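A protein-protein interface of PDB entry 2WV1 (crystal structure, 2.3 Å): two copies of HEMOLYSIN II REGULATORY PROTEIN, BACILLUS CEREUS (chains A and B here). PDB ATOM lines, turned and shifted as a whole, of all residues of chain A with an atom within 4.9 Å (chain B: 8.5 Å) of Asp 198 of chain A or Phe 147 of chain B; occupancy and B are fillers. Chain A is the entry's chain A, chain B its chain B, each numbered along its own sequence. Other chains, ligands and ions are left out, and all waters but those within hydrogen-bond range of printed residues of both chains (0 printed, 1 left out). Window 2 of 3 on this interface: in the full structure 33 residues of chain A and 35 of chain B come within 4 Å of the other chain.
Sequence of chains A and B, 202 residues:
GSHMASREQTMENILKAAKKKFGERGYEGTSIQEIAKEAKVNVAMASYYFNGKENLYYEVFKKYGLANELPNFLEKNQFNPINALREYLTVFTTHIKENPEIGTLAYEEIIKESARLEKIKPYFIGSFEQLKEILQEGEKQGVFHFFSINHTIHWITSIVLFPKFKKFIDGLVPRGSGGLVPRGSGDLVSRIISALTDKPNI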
ATOM      1  N   HIS A 145      22.770 -12.790 -12.693  1.00  0.00           N
ATOM      2  CA  HIS A 145      21.364 -12.937 -13.089  1.00  0.00           C
ATOM      3  C   HIS A 145      21.115 -14.400 -13.315  1.00  0.00           C
ATOM      4  O   HIS A 145      21.841 -15.050 -14.069  1.00  0.00           O
ATOM      5  CB  HIS A 145      21.056 -12.110 -14.355  1.00  0.00           C
ATOM      6  CG  HIS A 145      21.543 -10.698 -14.255  1.00  0.00           C
ATOM      7  ND1 HIS A 145      20.842  -9.715 -13.584  1.00  0.00           N
ATOM      8  CD2 HIS A 145      22.706 -10.125 -14.656  1.00  0.00           C
ATOM      9  CE1 HIS A 145      21.538  -8.590 -13.606  1.00  0.00           C
ATOM     10  NE2 HIS A 145      22.672  -8.811 -14.250  1.00  0.00           N
ATOM     11  N   ARG A 191      33.934 -18.850 -18.191  1.00  0.00           N
ATOM     12  CA  ARG A 191      32.687 -19.354 -18.756  1.00  0.00           C
ATOM     13  C   ARG A 191      31.568 -19.422 -17.722  1.00  0.00           C
ATOM     14  O   ARG A 191      30.450 -19.086 -18.016  1.00  0.00           O
ATOM     15  CB  ARG A 191      32.881 -20.718 -19.418  1.00  0.00           C
ATOM     16  CG  ARG A 191      33.772 -20.680 -20.623  1.00  0.00           C
ATOM     17  CD  ARG A 191      33.390 -21.826 -21.535  1.00  0.00           C
ATOM     18  NE  ARG A 191      34.090 -23.045 -21.164  1.00  0.00           N
ATOM     19  CZ  ARG A 191      33.664 -24.278 -21.439  1.00  0.00           C
ATOM     20  NH1 ARG A 191      32.508 -24.475 -22.077  1.00  0.00           N
ATOM     21  NH2 ARG A 191      34.400 -25.327 -21.058  1.00  0.00           N
ATOM     22  N   SER A 194      30.740 -15.620 -17.134  1.00  0.00           N
ATOM     23  CA  SER A 194      29.976 -15.120 -18.291  1.00  0.00           C
ATOM     24  C   SER A 194      28.506 -15.577 -18.291  1.00  0.00           C
ATOM     25  O   SER A 194      27.650 -14.821 -18.720  1.00  0.00           O
ATOM     26  CB  SER A 194      30.618 -15.546 -19.622  1.00  0.00           C
ATOM     27  OG  SER A 194      31.926 -15.030 -19.778  1.00  0.00           O
ATOM     28  N   ALA A 195      28.232 -16.809 -17.853  1.00  0.00           N
ATOM     29  CA  ALA A 195      26.857 -17.339 -17.824  1.00  0.00           C
ATOM     30  C   ALA A 195      26.022 -16.677 -16.723  1.00  0.00           C
ATOM     31  O   ALA A 195      24.807 -16.563 -16.842  1.00  0.00           O
ATOM     32  CB  ALA A 195      26.878 -18.843 -17.635  1.00  0.00           C
ATOM     33  N   LEU A 196      26.694 -16.225 -15.665  1.00  0.00           N
ATOM     34  CA  LEU A 196      26.052 -15.517 -14.556  1.00  0.00           C
ATOM     35  C   LEU A 196      25.821 -14.038 -14.816  1.00  0.00           C
ATOM     36  O   LEU A 196      24.853 -13.461 -14.299  1.00  0.00           O
ATOM     37  CB  LEU A 196      26.884 -15.692 -13.284  1.00  0.00           C
ATOM     38  CG  LEU A 196      26.955 -17.136 -12.785  1.00  0.00           C
ATOM     39  CD1 LEU A 196      27.965 -17.236 -11.684  1.00  0.00           C
ATOM     40  CD2 LEU A 196      25.590 -17.552 -12.274  1.00  0.00           C
ATOM     41  N   THR A 197      26.697 -13.414 -15.605  1.00  0.00           N
ATOM     42  CA  THR A 197      26.608 -11.972 -15.818  1.00  0.00           C
ATOM     43  C   THR A 197      25.799 -11.629 -17.068  1.00  0.00           C
ATOM     44  O   THR A 197      25.513 -10.465 -17.320  1.00  0.00           O
ATOM     45  CB  THR A 197      27.991 -11.307 -15.875  1.00  0.00           C
ATOM     46  OG1 THR A 197      28.723 -11.842 -16.980  1.00  0.00           O
ATOM     47  CG2 THR A 197      28.777 -11.585 -14.588  1.00  0.00           C
ATOM     48  N   ASP A 198      25.412 -12.657 -17.820  1.00  0.00           N
ATOM     49  CA  ASP A 198      24.647 -12.523 -19.062  1.00  0.00           C
ATOM     50  C   ASP A 198      23.288 -11.898 -18.800  1.00  0.00           C
ATOM     51  O   ASP A 198      22.470 -12.467 -18.086  1.00  0.00           O
ATOM     52  CB  ASP A 198      24.488 -13.910 -19.715  1.00  0.00           C
ATOM     53  CG  ASP A 198      23.707 -13.873 -21.035  1.00  0.00           C
ATOM     54  OD1 ASP A 198      23.871 -12.904 -21.801  1.00  0.00           O
ATOM     55  OD2 ASP A 198      22.939 -14.833 -21.311  1.00  0.00           O
ATOM     56  N   LYS A 199      23.062 -10.720 -19.375  1.00  0.00           N
ATOM     57  CA  LYS A 199      21.773 -10.031 -19.264  1.00  0.00           C
ATOM     58  C   LYS A 199      20.708 -10.663 -20.171  1.00  0.00           C
ATOM     59  O   LYS A 199      19.531 -10.278 -20.134  1.00  0.00           O
ATOM     60  CB  LYS A 199      21.929  -8.537 -19.585  1.00  0.00           C
ATOM     61  CG  LYS A 199      22.444  -7.709 -18.420  1.00  0.00           C
ATOM     62  CD  LYS A 199      23.337  -6.568 -18.902  1.00  0.00           C
ATOM     63  CE  LYS A 199      24.090  -5.928 -17.747  1.00  0.00           C
ATOM     64  NZ  LYS A 199      25.394  -5.415 -18.237  1.00  0.00           N
ATOM     65  N   GLU B 139      15.373 -21.001 -29.334  1.00  0.00           N
ATOM     66  CA  GLU B 139      16.048 -19.731 -29.199  1.00  0.00           C
ATOM     67  C   GLU B 139      15.641 -18.853 -30.375  1.00  0.00           C
ATOM     68  O   GLU B 139      15.205 -17.722 -30.183  1.00  0.00           O
ATOM     69  CB  GLU B 139      17.563 -19.913 -29.118  1.00  0.00           C
ATOM     70  CG  GLU B 139      18.373 -18.610 -29.295  1.00  0.00           C
ATOM     71  CD  GLU B 139      19.860 -18.840 -29.105  1.00  0.00           C
ATOM     72  OE1 GLU B 139      20.411 -19.763 -29.760  1.00  0.00           O
ATOM     73  OE2 GLU B 139      20.475 -18.118 -28.282  1.00  0.00           O
ATOM     74  N   PHE B 144      13.098 -19.736 -25.909  1.00  0.00           N
ATOM     75  CA  PHE B 144      14.135 -20.190 -24.977  1.00  0.00           C
ATOM     76  C   PHE B 144      15.189 -19.104 -24.865  1.00  0.00           C
ATOM     77  O   PHE B 144      15.530 -18.449 -25.863  1.00  0.00           O
ATOM     78  CB  PHE B 144      14.843 -21.461 -25.495  1.00  0.00           C
ATOM     79  CG  PHE B 144      13.968 -22.688 -25.531  1.00  0.00           C
ATOM     80  CD1 PHE B 144      12.940 -22.871 -24.602  1.00  0.00           C
ATOM     81  CD2 PHE B 144      14.219 -23.694 -26.458  1.00  0.00           C
ATOM     82  CE1 PHE B 144      12.142 -24.025 -24.629  1.00  0.00           C
ATOM     83  CE2 PHE B 144      13.442 -24.845 -26.495  1.00  0.00           C
ATOM     84  CZ  PHE B 144      12.388 -25.007 -25.578  1.00  0.00           C
ATOM     85  N   HIS B 145      15.734 -18.940 -23.668  1.00  0.00           N
ATOM     86  CA  HIS B 145      16.812 -17.982 -23.448  1.00  0.00           C
ATOM     87  C   HIS B 145      17.906 -18.658 -22.672  1.00  0.00           C
ATOM     88  O   HIS B 145      17.652 -19.216 -21.613  1.00  0.00           O
ATOM     89  CB  HIS B 145      16.281 -16.756 -22.696  1.00  0.00           C
ATOM     90  CG  HIS B 145      14.985 -16.260 -23.254  1.00  0.00           C
ATOM     91  ND1 HIS B 145      14.922 -15.388 -24.320  1.00  0.00           N
ATOM     92  CD2 HIS B 145      13.702 -16.583 -22.952  1.00  0.00           C
ATOM     93  CE1 HIS B 145      13.656 -15.159 -24.622  1.00  0.00           C
ATOM     94  NE2 HIS B 145      12.895 -15.867 -23.804  1.00  0.00           N
ATOM     95  N   PHE B 146      19.123 -18.630 -23.206  1.00  0.00           N
ATOM     96  CA  PHE B 146      20.239 -19.236 -22.512  1.00  0.00           C
ATOM     97  C   PHE B 146      21.512 -18.654 -23.030  1.00  0.00           C
ATOM     98  O   PHE B 146      21.551 -18.135 -24.148  1.00  0.00           O
ATOM     99  CB  PHE B 146      20.273 -20.748 -22.735  1.00  0.00           C
ATOM    100  CG  PHE B 146      20.114 -21.152 -24.179  1.00  0.00           C
ATOM    101  CD1 PHE B 146      18.875 -21.582 -24.661  1.00  0.00           C
ATOM    102  CD2 PHE B 146      21.189 -21.111 -25.051  1.00  0.00           C
ATOM    103  CE1 PHE B 146      18.717 -21.984 -25.992  1.00  0.00           C
ATOM    104  CE2 PHE B 146      21.040 -21.492 -26.387  1.00  0.00           C
ATOM    105  CZ  PHE B 146      19.805 -21.932 -26.853  1.00  0.00           C
ATOM    106  N   PHE B 147      22.571 -18.816 -22.247  1.00  0.00           N
ATOM    107  CA  PHE B 147      23.826 -18.152 -22.536  1.00  0.00           C
ATOM    108  C   PHE B 147      24.542 -18.758 -23.753  1.00  0.00           C
ATOM    109  O   PHE B 147      24.989 -18.029 -24.635  1.00  0.00           O
ATOM    110  CB  PHE B 147      24.671 -18.150 -21.270  1.00  0.00           C
ATOM    111  CG  PHE B 147      26.141 -18.008 -21.501  1.00  0.00           C
ATOM    112  CD1 PHE B 147      26.986 -19.114 -21.289  1.00  0.00           C
ATOM    113  CD2 PHE B 147      26.702 -16.767 -21.871  1.00  0.00           C
ATOM    114  CE1 PHE B 147      28.376 -19.006 -21.480  1.00  0.00           C
ATOM    115  CE2 PHE B 147      28.074 -16.644 -22.056  1.00  0.00           C
ATOM    116  CZ  PHE B 147      28.921 -17.774 -21.866  1.00  0.00           C
ATOM    117  N   SER B 148      24.628 -20.079 -23.789  1.00  0.00           N
ATOM    118  CA  SER B 148      25.189 -20.806 -24.925  1.00  0.00           C
ATOM    119  C   SER B 148      24.573 -22.186 -24.986  1.00  0.00           C
ATOM    120  O   SER B 148      24.066 -22.699 -24.005  1.00  0.00           O
ATOM    121  CB  SER B 148      26.708 -20.936 -24.818  1.00  0.00           C
ATOM    122  OG  SER B 148      27.104 -21.913 -23.847  1.00  0.00           O
ATOM    123  N   ILE B 149      24.648 -22.795 -26.153  1.00  0.00           N
ATOM    124  CA  ILE B 149      24.099 -24.100 -26.372  1.00  0.00           C
ATOM    125  C   ILE B 149      24.930 -25.121 -25.623  1.00  0.00           C
ATOM    126  O   ILE B 149      24.380 -26.067 -25.051  1.00  0.00           O
ATOM    127  CB  ILE B 149      24.037 -24.416 -27.891  1.00  0.00           C
ATOM    128  CG1 ILE B 149      22.971 -25.459 -28.168  1.00  0.00           C
ATOM    129  CG2 ILE B 149      25.376 -24.887 -28.425  1.00  0.00           C
ATOM    130  CD1 ILE B 149      21.600 -24.843 -28.261  1.00  0.00           C
ATOM    131  N   ASN B 150      26.252 -24.929 -25.611  1.00  0.00           N
ATOM    132  CA  ASN B 150      27.139 -25.864 -24.916  1.00  0.00           C
ATOM    133  C   ASN B 150      26.836 -25.940 -23.425  1.00  0.00           C
ATOM    134  O   ASN B 150      26.698 -27.024 -22.865  1.00  0.00           O
ATOM    135  CB  ASN B 150      28.606 -25.517 -25.149  1.00  0.00           C
ATOM    136  CG  ASN B 150      29.526 -26.290 -24.236  1.00  0.00           C
ATOM    137  OD1 ASN B 150      29.593 -26.019 -23.039  1.00  0.00           O
ATOM    138  ND2 ASN B 150      30.241 -27.267 -24.791  1.00  0.00           N
ATOM    139  N   HIS B 151      26.717 -24.778 -22.787  1.00  0.00           N
ATOM    140  CA  HIS B 151      26.395 -24.688 -21.355  1.00  0.00           C
ATOM    141  C   HIS B 151      25.070 -25.384 -21.041  1.00  0.00           C
ATOM    142  O   HIS B 151      24.955 -26.174 -20.107  1.00  0.00           O
ATOM    143  CB  HIS B 151      26.350 -23.207 -20.963  1.00  0.00           C
ATOM    144  CG  HIS B 151      25.653 -22.925 -19.674  1.00  0.00           C
ATOM    145  ND1 HIS B 151      26.327 -22.800 -18.480  1.00  0.00           N
ATOM    146  CD2 HIS B 151      24.347 -22.685 -19.400  1.00  0.00           C
ATOM    147  CE1 HIS B 151      25.459 -22.523 -17.518  1.00  0.00           C
ATOM    148  NE2 HIS B 151      24.254 -22.440 -18.053  1.00  0.00           N
ATOM    149  N   THR B 152      24.073 -25.089 -21.850  1.00  0.00           N
ATOM    150  CA  THR B 152      22.729 -25.640 -21.690  1.00  0.00           C
ATOM    151  C   THR B 152      22.634 -27.155 -21.904  1.00  0.00           C
ATOM    152  O   THR B 152      21.951 -27.837 -21.162  1.00  0.00           O
ATOM    153  CB  THR B 152      21.771 -24.949 -22.686  1.00  0.00           C
ATOM    154  OG1 THR B 152      21.907 -23.552 -22.505  1.00  0.00           O
ATOM    155  CG2 THR B 152      20.324 -25.354 -22.427  1.00  0.00           C
ATOM    156  N   TRP B 155      24.097 -28.766 -18.646  1.00  0.00           N
ATOM    157  CA  TRP B 155      23.255 -28.953 -17.471  1.00  0.00           C
ATOM    158  C   TRP B 155      21.993 -29.782 -17.719  1.00  0.00           C
ATOM    159  O   TRP B 155      21.530 -30.480 -16.821  1.00  0.00           O
ATOM    160  CB  TRP B 155      22.994 -27.666 -16.674  1.00  0.00           C
ATOM    161  CG  TRP B 155      22.170 -26.627 -17.374  1.00  0.00           C
ATOM    162  CD1 TRP B 155      22.635 -25.520 -18.043  1.00  0.00           C
ATOM    163  CD2 TRP B 155      20.741 -26.565 -17.439  1.00  0.00           C
ATOM    164  NE1 TRP B 155      21.580 -24.777 -18.531  1.00  0.00           N
ATOM    165  CE2 TRP B 155      20.405 -25.401 -18.187  1.00  0.00           C
ATOM    166  CE3 TRP B 155      19.708 -27.369 -16.935  1.00  0.00           C
ATOM    167  CZ2 TRP B 155      19.078 -25.026 -18.445  1.00  0.00           C
ATOM    168  CZ3 TRP B 155      18.375 -27.001 -17.205  1.00  0.00           C
ATOM    169  CH2 TRP B 155      18.078 -25.846 -17.965  1.00  0.00           C
ATOM    170  N   ALA B 195      13.569 -22.958 -16.528  1.00  0.00           N
ATOM    171  CA  ALA B 195      14.890 -22.312 -16.579  1.00  0.00           C
ATOM    172  C   ALA B 195      15.144 -21.757 -17.980  1.00  0.00           C
ATOM    173  O   ALA B 195      15.829 -20.740 -18.136  1.00  0.00           O
ATOM    174  CB  ALA B 195      16.018 -23.268 -16.148  1.00  0.00           C
ATOM    175  N   LEU B 196      14.554 -22.403 -18.986  1.00  0.00           N
ATOM    176  CA  LEU B 196      14.733 -21.964 -20.372  1.00  0.00           C
ATOM    177  C   LEU B 196      13.798 -20.833 -20.825  1.00  0.00           C
ATOM    178  O   LEU B 196      14.147 -20.048 -21.733  1.00  0.00           O
ATOM    179  CB  LEU B 196      14.595 -23.143 -21.330  1.00  0.00           C
ATOM    180  CG  LEU B 196      15.687 -24.203 -21.274  1.00  0.00           C
ATOM    181  CD1 LEU B 196      15.236 -25.364 -22.113  1.00  0.00           C
ATOM    182  CD2 LEU B 196      17.024 -23.673 -21.744  1.00  0.00           C
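Phe 147 of chain B touches Ser 194 of chain A (CZ to CB, 3.6 Å). Phe 147 of chain B touches Ala 195 of chain A (CD1 to CB, 3.7 Å). CB of Ala 195 of chain A touches CE1 of His 151 of chain B (3.9 Å). OD2 of Asp 198 of chain A touches CA of Phe 147 of chain B (3.6 Å).
Printed residues of chain B within 4 Å of Asp 198 of chain A: Phe 147. Of chain B, only Phe 147 (3.7 Å) and His 151 (3.9 Å) come within 4 Å of Ala 195 of chain A. Of the printed residues of chain B, Ser 194 of chain A touches Phe 147 (3.6 Å). Of the printed residues of chain B, Arg 191 of chain A touches Asn 150 (3.4 Å). Of the printed residues of chain A, Asn 150 of chain B touches Arg 191. Thr 197 of chain A touches none of the printed residues of chain B. His 145 of chain B touches none of the printed residues of chain A. The nearest residue of chain B that does not touch Asp 198 of chain A is Phe 146 of chain B (4.4 Å).
3 positions are printed for both chains.
The side-chain amide oxygen (OD1) of Asn 150 of chain B is in hydrogen-bond range of the guanidinium group (NH1) of Arg 191 of chain A (3.4 Å).
The side-chain hydroxyl (OG) of Ser 148 of chain B sits at hydrogen-bond distance from the backbone NH (N) of His 151 of chain B, 3.1 Å away.
Hydrophobic or aromatic side chains of chain A that line the printed part of chain B: Ala 195. Along chain A the printed residues that touch a printed residue of chain B span positions 191 to 198. Among the printed residues, no Asp or Glu carboxylate lies within 4 Å of a Lys or Arg side-chain nitrogen of the other chain.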
